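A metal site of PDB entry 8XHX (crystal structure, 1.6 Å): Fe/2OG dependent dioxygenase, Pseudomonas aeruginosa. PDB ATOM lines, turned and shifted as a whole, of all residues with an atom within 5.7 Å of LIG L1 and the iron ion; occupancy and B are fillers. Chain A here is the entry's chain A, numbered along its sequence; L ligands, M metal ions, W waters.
The iron ion is bound by O2 of LIG L1, NE2 of His 172, O3 of LIG L1, OD1 of Asp 174, NE2 of His 230 and water W3. The iron ion has six donor atoms within binding distance.
OD2 of Asp 174 lies within hydrogen-bond range of ND2 of Asn 209. OD2 of Asp 174 is in hydrogen-bond range of OG1 of Thr 179 (2.7 Å). The backbone NH (N) of Asn 158 lies within hydrogen-bond range of the backbone carbonyl oxygen (O) of Ser 244 (2.8 Å). The backbone carbonyl oxygen (O) of Arg 242 is in hydrogen-bond range of the backbone NH (N) of Phe 160 (3.0 Å). The side-chain amide oxygen of Asn 158 lies within hydrogen-bond range of the side-chain amide nitrogen of Gln 94, 2.9 Å away. The backbone NH (N) of Leu 169 sits at hydrogen-bond distance from the backbone carbonyl oxygen (O) of Val 232 (3.1 Å).
An oxygen (O5) of LIG L1 sits at hydrogen-bond distance from the side-chain hydroxyl (OG) of Ser 244 (2.6 Å). NH1 of Arg 242 lies within salt-bridge range of O5 of LIG L1 (2.8 Å). The side-chain amide nitrogen (ND2) of Asn 158 sits at hydrogen-bond distance from an oxygen (O1) of LIG L1 (2.9 Å). O2 of LG2 L2 sits at hydrogen-bond distance from OG1 of Thr 156 (2.8 Å).
Of the 22 residues printed, 3 come within 4 Å of the iron ion. The nearest printed residue that does not touch the iron ion is Phe 248 (4.6 Å).
Water W3 bridges OD2 of Asp 174 (2.6 Å) and OD1 of Asn 209 (3.4 Å). Water W1 lies within hydrogen-bond range of OG of Ser 183 (2.7 Å), O4 of LIG L1 (2.8 Å) and NH2 of Arg 242 (3.2 Å).
Merely in contact with LIG L1: Phe 160 (3.6 Å), Leu 169 (3.7 Å), Leu 181 (3.8 Å), Leu 188 (3.7 Å), Val 232 (3.6 Å) and Phe 248 (3.4 Å). Hydrophobic or aromatic side chains within 4 Å of LIG L1: Phe 160, Leu 169, His 172, Leu 181, Leu 188, His 230, Val 232 and Phe 248. Of the 22 residues printed, 12 come within 4 Å of LIG L1. The nearest printed residue that does not touch LIG L1 is Ser 183 (4.6 Å).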
ATOM      1  N   GLN A  94     -32.223  14.626  20.918  1.00  0.00           N
ATOM      2  CA  GLN A  94     -30.855  15.044  20.623  1.00  0.00           C
ATOM      3  C   GLN A  94     -30.739  16.560  20.622  1.00  0.00           C
ATOM      4  O   GLN A  94     -31.704  17.286  20.401  1.00  0.00           O
ATOM      5  CB  GLN A  94     -30.417  14.504  19.264  1.00  0.00           C
ATOM      6  CG  GLN A  94     -30.322  12.986  19.227  1.00  0.00           C
ATOM      7  CD  GLN A  94     -30.136  12.468  17.814  1.00  0.00           C
ATOM      8  OE1 GLN A  94     -30.899  12.829  16.910  1.00  0.00           O
ATOM      9  NE2 GLN A  94     -29.113  11.644  17.607  1.00  0.00           N
ATOM     10  N   THR A 156     -22.642  17.276  19.888  1.00  0.00           N
ATOM     11  CA  THR A 156     -23.982  16.708  19.726  1.00  0.00           C
ATOM     12  C   THR A 156     -24.280  15.782  20.888  1.00  0.00           C
ATOM     13  O   THR A 156     -23.445  14.940  21.236  1.00  0.00           O
ATOM     14  CB  THR A 156     -24.096  15.967  18.397  1.00  0.00           C
ATOM     15  OG1 THR A 156     -24.077  16.911  17.326  1.00  0.00           O
ATOM     16  CG2 THR A 156     -25.407  15.167  18.340  1.00  0.00           C
ATOM     17  N   ASN A 158     -26.916  13.048  22.948  1.00  0.00           N
ATOM     18  CA  ASN A 158     -27.941  12.008  22.887  1.00  0.00           C
ATOM     19  C   ASN A 158     -28.485  11.809  24.294  1.00  0.00           C
ATOM     20  O   ASN A 158     -27.704  11.501  25.205  1.00  0.00           O
ATOM     21  CB  ASN A 158     -27.370  10.678  22.395  1.00  0.00           C
ATOM     22  CG  ASN A 158     -26.899  10.726  20.963  1.00  0.00           C
ATOM     23  OD1 ASN A 158     -27.653  11.107  20.072  1.00  0.00           O
ATOM     24  ND2 ASN A 158     -25.655  10.328  20.748  1.00  0.00           N
ATOM     25  N   PHE A 160     -31.108   9.146  25.854  1.00  0.00           N
ATOM     26  CA  PHE A 160     -31.854   7.936  25.507  1.00  0.00           C
ATOM     27  C   PHE A 160     -33.088   7.856  26.390  1.00  0.00           C
ATOM     28  O   PHE A 160     -32.989   7.532  27.572  1.00  0.00           O
ATOM     29  CB  PHE A 160     -30.962   6.698  25.638  1.00  0.00           C
ATOM     30  CG  PHE A 160     -29.844   6.668  24.628  1.00  0.00           C
ATOM     31  CD1 PHE A 160     -29.969   5.926  23.460  1.00  0.00           C
ATOM     32  CD2 PHE A 160     -28.693   7.413  24.828  1.00  0.00           C
ATOM     33  CE1 PHE A 160     -28.941   5.929  22.508  1.00  0.00           C
ATOM     34  CE2 PHE A 160     -27.663   7.414  23.893  1.00  0.00           C
ATOM     35  CZ  PHE A 160     -27.790   6.680  22.732  1.00  0.00           C
ATOM     36  N   LEU A 169     -30.441   3.785  19.291  1.00  0.00           N
ATOM     37  CA  LEU A 169     -30.022   4.612  18.166  1.00  0.00           C
ATOM     38  C   LEU A 169     -29.778   3.675  17.002  1.00  0.00           C
ATOM     39  O   LEU A 169     -29.070   2.672  17.156  1.00  0.00           O
ATOM     40  CB  LEU A 169     -28.761   5.410  18.506  1.00  0.00           C
ATOM     41  CG  LEU A 169     -28.163   6.266  17.374  1.00  0.00           C
ATOM     42  CD1 LEU A 169     -29.189   7.254  16.874  1.00  0.00           C
ATOM     43  CD2 LEU A 169     -26.916   6.987  17.850  1.00  0.00           C
ATOM     44  N   HIS A 172     -25.852   3.073  11.946  1.00  0.00           N
ATOM     45  CA  HIS A 172     -25.389   4.183  11.114  1.00  0.00           C
ATOM     46  C   HIS A 172     -23.866   4.156  11.023  1.00  0.00           C
ATOM     47  O   HIS A 172     -23.186   3.512  11.827  1.00  0.00           O
ATOM     48  CB  HIS A 172     -25.845   5.533  11.678  1.00  0.00           C
ATOM     49  CG  HIS A 172     -25.204   5.869  12.998  1.00  0.00           C
ATOM     50  ND1 HIS A 172     -25.628   5.326  14.194  1.00  0.00           N
ATOM     51  CD2 HIS A 172     -24.158   6.675  13.295  1.00  0.00           C
ATOM     52  CE1 HIS A 172     -24.872   5.793  15.174  1.00  0.00           C
ATOM     53  NE2 HIS A 172     -23.973   6.614  14.656  1.00  0.00           N
ATOM     54  N   LYS A 173     -23.357   4.901  10.054  1.00  0.00           N
ATOM     55  CA  LYS A 173     -21.982   5.378  10.085  1.00  0.00           C
ATOM     56  C   LYS A 173     -22.015   6.866  10.350  1.00  0.00           C
ATOM     57  O   LYS A 173     -22.960   7.542   9.935  1.00  0.00           O
ATOM     58  CB  LYS A 173     -21.270   5.102   8.754  1.00  0.00           C
ATOM     59  CG  LYS A 173     -20.951   3.631   8.511  1.00  0.00           C
ATOM     60  CD  LYS A 173     -20.344   3.441   7.103  1.00  0.00           C
ATOM     61  CE  LYS A 173     -19.994   1.983   6.828  1.00  0.00           C
ATOM     62  NZ  LYS A 173     -19.437   1.828   5.442  1.00  0.00           N
ATOM     63  N   ASP A 174     -21.033   7.368  11.094  1.00  0.00           N
ATOM     64  CA  ASP A 174     -20.891   8.807  11.241  1.00  0.00           C
ATOM     65  C   ASP A 174     -20.453   9.407   9.901  1.00  0.00           C
ATOM     66  O   ASP A 174     -19.846   8.731   9.061  1.00  0.00           O
ATOM     67  CB  ASP A 174     -19.865   9.161  12.317  1.00  0.00           C
ATOM     68  CG  ASP A 174     -20.289   8.735  13.716  1.00  0.00           C
ATOM     69  OD1 ASP A 174     -21.425   8.249  13.929  1.00  0.00           O
ATOM     70  OD2 ASP A 174     -19.458   8.899  14.635  1.00  0.00           O
ATOM     71  N   THR A 179     -14.776  11.167  15.186  1.00  0.00           N
ATOM     72  CA  THR A 179     -15.738  11.471  16.236  1.00  0.00           C
ATOM     73  C   THR A 179     -15.066  11.134  17.559  1.00  0.00           C
ATOM     74  O   THR A 179     -14.506  10.040  17.705  1.00  0.00           O
ATOM     75  CB  THR A 179     -16.995  10.618  16.072  1.00  0.00           C
ATOM     76  OG1 THR A 179     -17.600  10.898  14.799  1.00  0.00           O
ATOM     77  CG2 THR A 179     -17.988  10.887  17.194  1.00  0.00           C
ATOM     78  N   LEU A 181     -15.992  10.509  21.308  1.00  0.00           N
ATOM     79  CA  LEU A 181     -17.247  10.166  21.973  1.00  0.00           C
ATOM     80  C   LEU A 181     -17.081  10.062  23.491  1.00  0.00           C
ATOM     81  O   LEU A 181     -16.215   9.315  23.971  1.00  0.00           O
ATOM     82  CB  LEU A 181     -17.808   8.853  21.419  1.00  0.00           C
ATOM     83  CG  LEU A 181     -19.001   8.195  22.136  1.00  0.00           C
ATOM     84  CD1 LEU A 181     -20.286   9.047  21.968  1.00  0.00           C
ATOM     85  CD2 LEU A 181     -19.205   6.801  21.539  1.00  0.00           C
ATOM     86  N   SER A 183     -18.931   8.830  26.772  1.00  0.00           N
ATOM     87  CA  SER A 183     -20.015   8.010  27.277  1.00  0.00           C
ATOM     88  C   SER A 183     -19.580   7.312  28.553  1.00  0.00           C
ATOM     89  O   SER A 183     -18.389   7.241  28.865  1.00  0.00           O
ATOM     90  CB  SER A 183     -20.484   6.978  26.236  1.00  0.00           C
ATOM     91  OG  SER A 183     -19.375   6.192  25.779  1.00  0.00           O
ATOM     92  N   GLY A 187     -23.982  -0.165  25.764  1.00  0.00           N
ATOM     93  CA  GLY A 187     -25.054   0.076  24.821  1.00  0.00           C
ATOM     94  C   GLY A 187     -24.554   0.169  23.394  1.00  0.00           C
ATOM     95  O   GLY A 187     -25.224  -0.271  22.456  1.00  0.00           O
ATOM     96  N   LEU A 188     -23.379   0.762  23.214  1.00  0.00           N
ATOM     97  CA  LEU A 188     -22.764   0.844  21.892  1.00  0.00           C
ATOM     98  C   LEU A 188     -22.358  -0.546  21.414  1.00  0.00           C
ATOM     99  O   LEU A 188     -21.738  -1.306  22.159  1.00  0.00           O
ATOM    100  CB  LEU A 188     -21.543   1.768  21.926  1.00  0.00           C
ATOM    101  CG  LEU A 188     -20.706   1.864  20.641  1.00  0.00           C
ATOM    102  CD1 LEU A 188     -21.512   2.567  19.545  1.00  0.00           C
ATOM    103  CD2 LEU A 188     -19.411   2.618  20.920  1.00  0.00           C
ATOM    104  N   ASN A 209     -13.934   7.219  16.601  1.00  0.00           N
ATOM    105  CA  ASN A 209     -14.225   6.411  15.423  1.00  0.00           C
ATOM    106  C   ASN A 209     -14.125   7.253  14.172  1.00  0.00           C
ATOM    107  O   ASN A 209     -14.152   8.488  14.216  1.00  0.00           O
ATOM    108  CB  ASN A 209     -15.596   5.711  15.524  1.00  0.00           C
ATOM    109  CG  ASN A 209     -16.752   6.675  15.528  1.00  0.00           C
ATOM    110  OD1 ASN A 209     -17.223   7.095  16.589  1.00  0.00           O
ATOM    111  ND2 ASN A 209     -17.262   6.992  14.348  1.00  0.00           N
ATOM    112  N   HIS A 230     -22.444   1.213  13.408  1.00  0.00           N
ATOM    113  CA  HIS A 230     -22.590   1.020  14.838  1.00  0.00           C
ATOM    114  C   HIS A 230     -23.998   1.441  15.232  1.00  0.00           C
ATOM    115  O   HIS A 230     -24.705   2.108  14.469  1.00  0.00           O
ATOM    116  CB  HIS A 230     -21.511   1.777  15.641  1.00  0.00           C
ATOM    117  CG  HIS A 230     -21.386   3.226  15.298  1.00  0.00           C
ATOM    118  ND1 HIS A 230     -20.797   3.670  14.122  1.00  0.00           N
ATOM    119  CD2 HIS A 230     -21.716   4.341  15.999  1.00  0.00           C
ATOM    120  CE1 HIS A 230     -20.821   4.995  14.102  1.00  0.00           C
ATOM    121  NE2 HIS A 230     -21.356   5.420  15.227  1.00  0.00           N
ATOM    122  N   ARG A 231     -24.400   1.059  16.444  1.00  0.00           N
ATOM    123  CA  ARG A 231     -25.766   1.246  16.918  1.00  0.00           C
ATOM    124  C   ARG A 231     -25.740   1.301  18.436  1.00  0.00           C
ATOM    125  O   ARG A 231     -24.728   0.982  19.059  1.00  0.00           O
ATOM    126  CB  ARG A 231     -26.685   0.108  16.445  1.00  0.00           C
ATOM    127  CG  ARG A 231     -26.326  -1.227  17.064  1.00  0.00           C
ATOM    128  CD  ARG A 231     -27.121  -2.401  16.487  1.00  0.00           C
ATOM    129  NE  ARG A 231     -26.904  -3.589  17.310  1.00  0.00           N
ATOM    130  CZ  ARG A 231     -27.307  -4.810  16.975  1.00  0.00           C
ATOM    131  NH1 ARG A 231     -27.940  -5.000  15.830  1.00  0.00           N
ATOM    132  NH2 ARG A 231     -27.063  -5.837  17.783  1.00  0.00           N
ATOM    133  N   VAL A 232     -26.859   1.714  19.044  1.00  0.00           N
ATOM    134  CA  VAL A 232     -27.031   1.647  20.482  1.00  0.00           C
ATOM    135  C   VAL A 232     -28.272   0.820  20.799  1.00  0.00           C
ATOM    136  O   VAL A 232     -29.364   1.103  20.279  1.00  0.00           O
ATOM    137  CB  VAL A 232     -27.118   3.041  21.140  1.00  0.00           C
ATOM    138  CG1 VAL A 232     -27.275   2.902  22.658  1.00  0.00           C
ATOM    139  CG2 VAL A 232     -25.852   3.849  20.836  1.00  0.00           C
ATOM    140  N   ARG A 242     -29.517   6.685  30.018  1.00  0.00           N
ATOM    141  CA  ARG A 242     -28.231   6.759  29.349  1.00  0.00           C
ATOM    142  C   ARG A 242     -28.129   8.065  28.589  1.00  0.00           C
ATOM    143  O   ARG A 242     -29.123   8.557  28.042  1.00  0.00           O
ATOM    144  CB  ARG A 242     -28.083   5.582  28.379  1.00  0.00           C
ATOM    145  CG  ARG A 242     -26.691   5.433  27.798  1.00  0.00           C
ATOM    146  CD  ARG A 242     -26.640   4.210  26.891  1.00  0.00           C
ATOM    147  NE  ARG A 242     -25.271   3.928  26.444  1.00  0.00           N
ATOM    148  CZ  ARG A 242     -24.683   4.535  25.422  1.00  0.00           C
ATOM    149  NH1 ARG A 242     -25.326   5.461  24.718  1.00  0.00           N
ATOM    150  NH2 ARG A 242     -23.431   4.199  25.099  1.00  0.00           N
ATOM    151  N   PHE A 243     -26.920   8.636  28.560  1.00  0.00           N
ATOM    152  CA  PHE A 243     -26.615   9.740  27.657  1.00  0.00           C
ATOM    153  C   PHE A 243     -25.271   9.495  27.000  1.00  0.00           C
ATOM    154  O   PHE A 243     -24.454   8.699  27.472  1.00  0.00           O
ATOM    155  CB  PHE A 243     -26.601  11.122  28.358  1.00  0.00           C
ATOM    156  CG  PHE A 243     -25.489  11.301  29.376  1.00  0.00           C
ATOM    157  CD1 PHE A 243     -24.210  11.683  28.975  1.00  0.00           C
ATOM    158  CD2 PHE A 243     -25.728  11.128  30.728  1.00  0.00           C
ATOM    159  CE1 PHE A 243     -23.195  11.868  29.898  1.00  0.00           C
ATOM    160  CE2 PHE A 243     -24.714  11.314  31.651  1.00  0.00           C
ATOM    161  CZ  PHE A 243     -23.440  11.683  31.232  1.00  0.00           C
ATOM    162  N   SER A 244     -25.041  10.207  25.895  1.00  0.00           N
ATOM    163  CA  SER A 244     -23.705  10.281  25.330  1.00  0.00           C
ATOM    164  C   SER A 244     -23.608  11.614  24.613  1.00  0.00           C
ATOM    165  O   SER A 244     -24.623  12.245  24.298  1.00  0.00           O
ATOM    166  CB  SER A 244     -23.411   9.123  24.368  1.00  0.00           C
ATOM    167  OG  SER A 244     -24.341   9.106  23.294  1.00  0.00           O
ATOM    168  N   ALA A 246     -20.703  13.838  21.749  1.00  0.00           N
ATOM    169  CA  ALA A 246     -19.474  13.646  21.002  1.00  0.00           C
ATOM    170  C   ALA A 246     -19.145  14.896  20.220  1.00  0.00           C
ATOM    171  O   ALA A 246     -20.023  15.694  19.875  1.00  0.00           O
ATOM    172  CB  ALA A 246     -19.579  12.436  20.049  1.00  0.00           C
ATOM    173  N   PHE A 248     -18.025  15.819  16.719  1.00  0.00           N
ATOM    174  CA  PHE A 248     -17.965  15.304  15.354  1.00  0.00           C
ATOM    175  C   PHE A 248     -17.203  16.290  14.490  1.00  0.00           C
ATOM    176  O   PHE A 248     -17.576  17.457  14.427  1.00  0.00           O
ATOM    177  CB  PHE A 248     -19.373  15.110  14.765  1.00  0.00           C
ATOM    178  CG  PHE A 248     -20.200  14.066  15.464  1.00  0.00           C
ATOM    179  CD1 PHE A 248     -20.286  12.784  14.947  1.00  0.00           C
ATOM    180  CD2 PHE A 248     -20.898  14.372  16.620  1.00  0.00           C
ATOM    181  CE1 PHE A 248     -21.057  11.813  15.585  1.00  0.00           C
ATOM    182  CE2 PHE A 248     -21.662  13.406  17.269  1.00  0.00           C
ATOM    183  CZ  PHE A 248     -21.742  12.124  16.740  1.00  0.00           C
HETATM  184  C1  LIG L   1     -23.554   8.912  17.669  1.00  0.00           C
HETATM  185  O1  LIG L   1     -24.078   9.845  18.325  1.00  0.00           O
HETATM  186  O2  LIG L   1     -23.240   9.035  16.466  1.00  0.00           O
HETATM  187  C2  LIG L   1     -23.302   7.642  18.321  1.00  0.00           C
HETATM  188  O3  LIG L   1     -22.894   6.723  17.631  1.00  0.00           O
HETATM  189  C3  LIG L   1     -23.560   7.500  19.812  1.00  0.00           C
HETATM  190  C4  LIG L   1     -23.001   6.193  20.403  1.00  0.00           C
HETATM  191  C5  LIG L   1     -23.261   6.036  21.894  1.00  0.00           C
HETATM  192  O4  LIG L   1     -22.515   5.256  22.536  1.00  0.00           O
HETATM  193  O5  LIG L   1     -24.222   6.644  22.418  1.00  0.00           O
HETATM  194  C1  LG2 L   2     -22.628  15.185  12.661  1.00  0.00           C
HETATM  195  C2  LG2 L   2     -23.223  14.931  14.036  1.00  0.00           C
HETATM  196  C3  LG2 L   2     -23.733  12.446  13.529  1.00  0.00           C
HETATM  197  C4  LG2 L   2     -22.893  12.640  12.276  1.00  0.00           C
HETATM  198  C5  LG2 L   2     -25.183  12.177  13.110  1.00  0.00           C
HETATM  199  C6  LG2 L   2     -23.495  16.193  11.892  1.00  0.00           C
HETATM  200  C7  LG2 L   2     -25.906  11.101  13.931  1.00  0.00           C
HETATM  201  C8  LG2 L   2     -25.981  11.476  15.410  1.00  0.00           C
HETATM  202  C9  LG2 L   2     -25.242   9.736  13.786  1.00  0.00           C
HETATM  203  C10 LG2 L   2     -22.776  16.560  10.584  1.00  0.00           C
HETATM  204  C11 LG2 L   2     -24.874  15.617  11.624  1.00  0.00           C
HETATM  205  C12 LG2 L   2     -25.797  16.603  10.892  1.00  0.00           C
HETATM  206  N1  LG2 L   2     -22.380  13.967  11.882  1.00  0.00           N
HETATM  207  N2  LG2 L   2     -23.714  13.623  14.416  1.00  0.00           N
HETATM  208  O1  LG2 L   2     -22.637  11.671  11.622  1.00  0.00           O
HETATM  209  O2  LG2 L   2     -23.253  15.835  14.826  1.00  0.00           O
HETATM  210  O3  LG2 L   2     -27.212  11.007  13.447  1.00  0.00           O
HETATM  211  O4  LG2 L   2     -25.968  17.784  11.615  1.00  0.00           O
HETATM  212 FE    FE M   1     -22.273   7.380  15.694  1.00  0.00          FE
HETATM  213  O   HOH W   1     -20.348   4.316  24.110  1.00  0.00           O
HETATM  214  O   HOH W   2     -19.538   6.079  18.336  1.00  0.00           O
HETATM  215  O   HOH W   3     -20.483   8.026  16.826  1.00  0.00           O
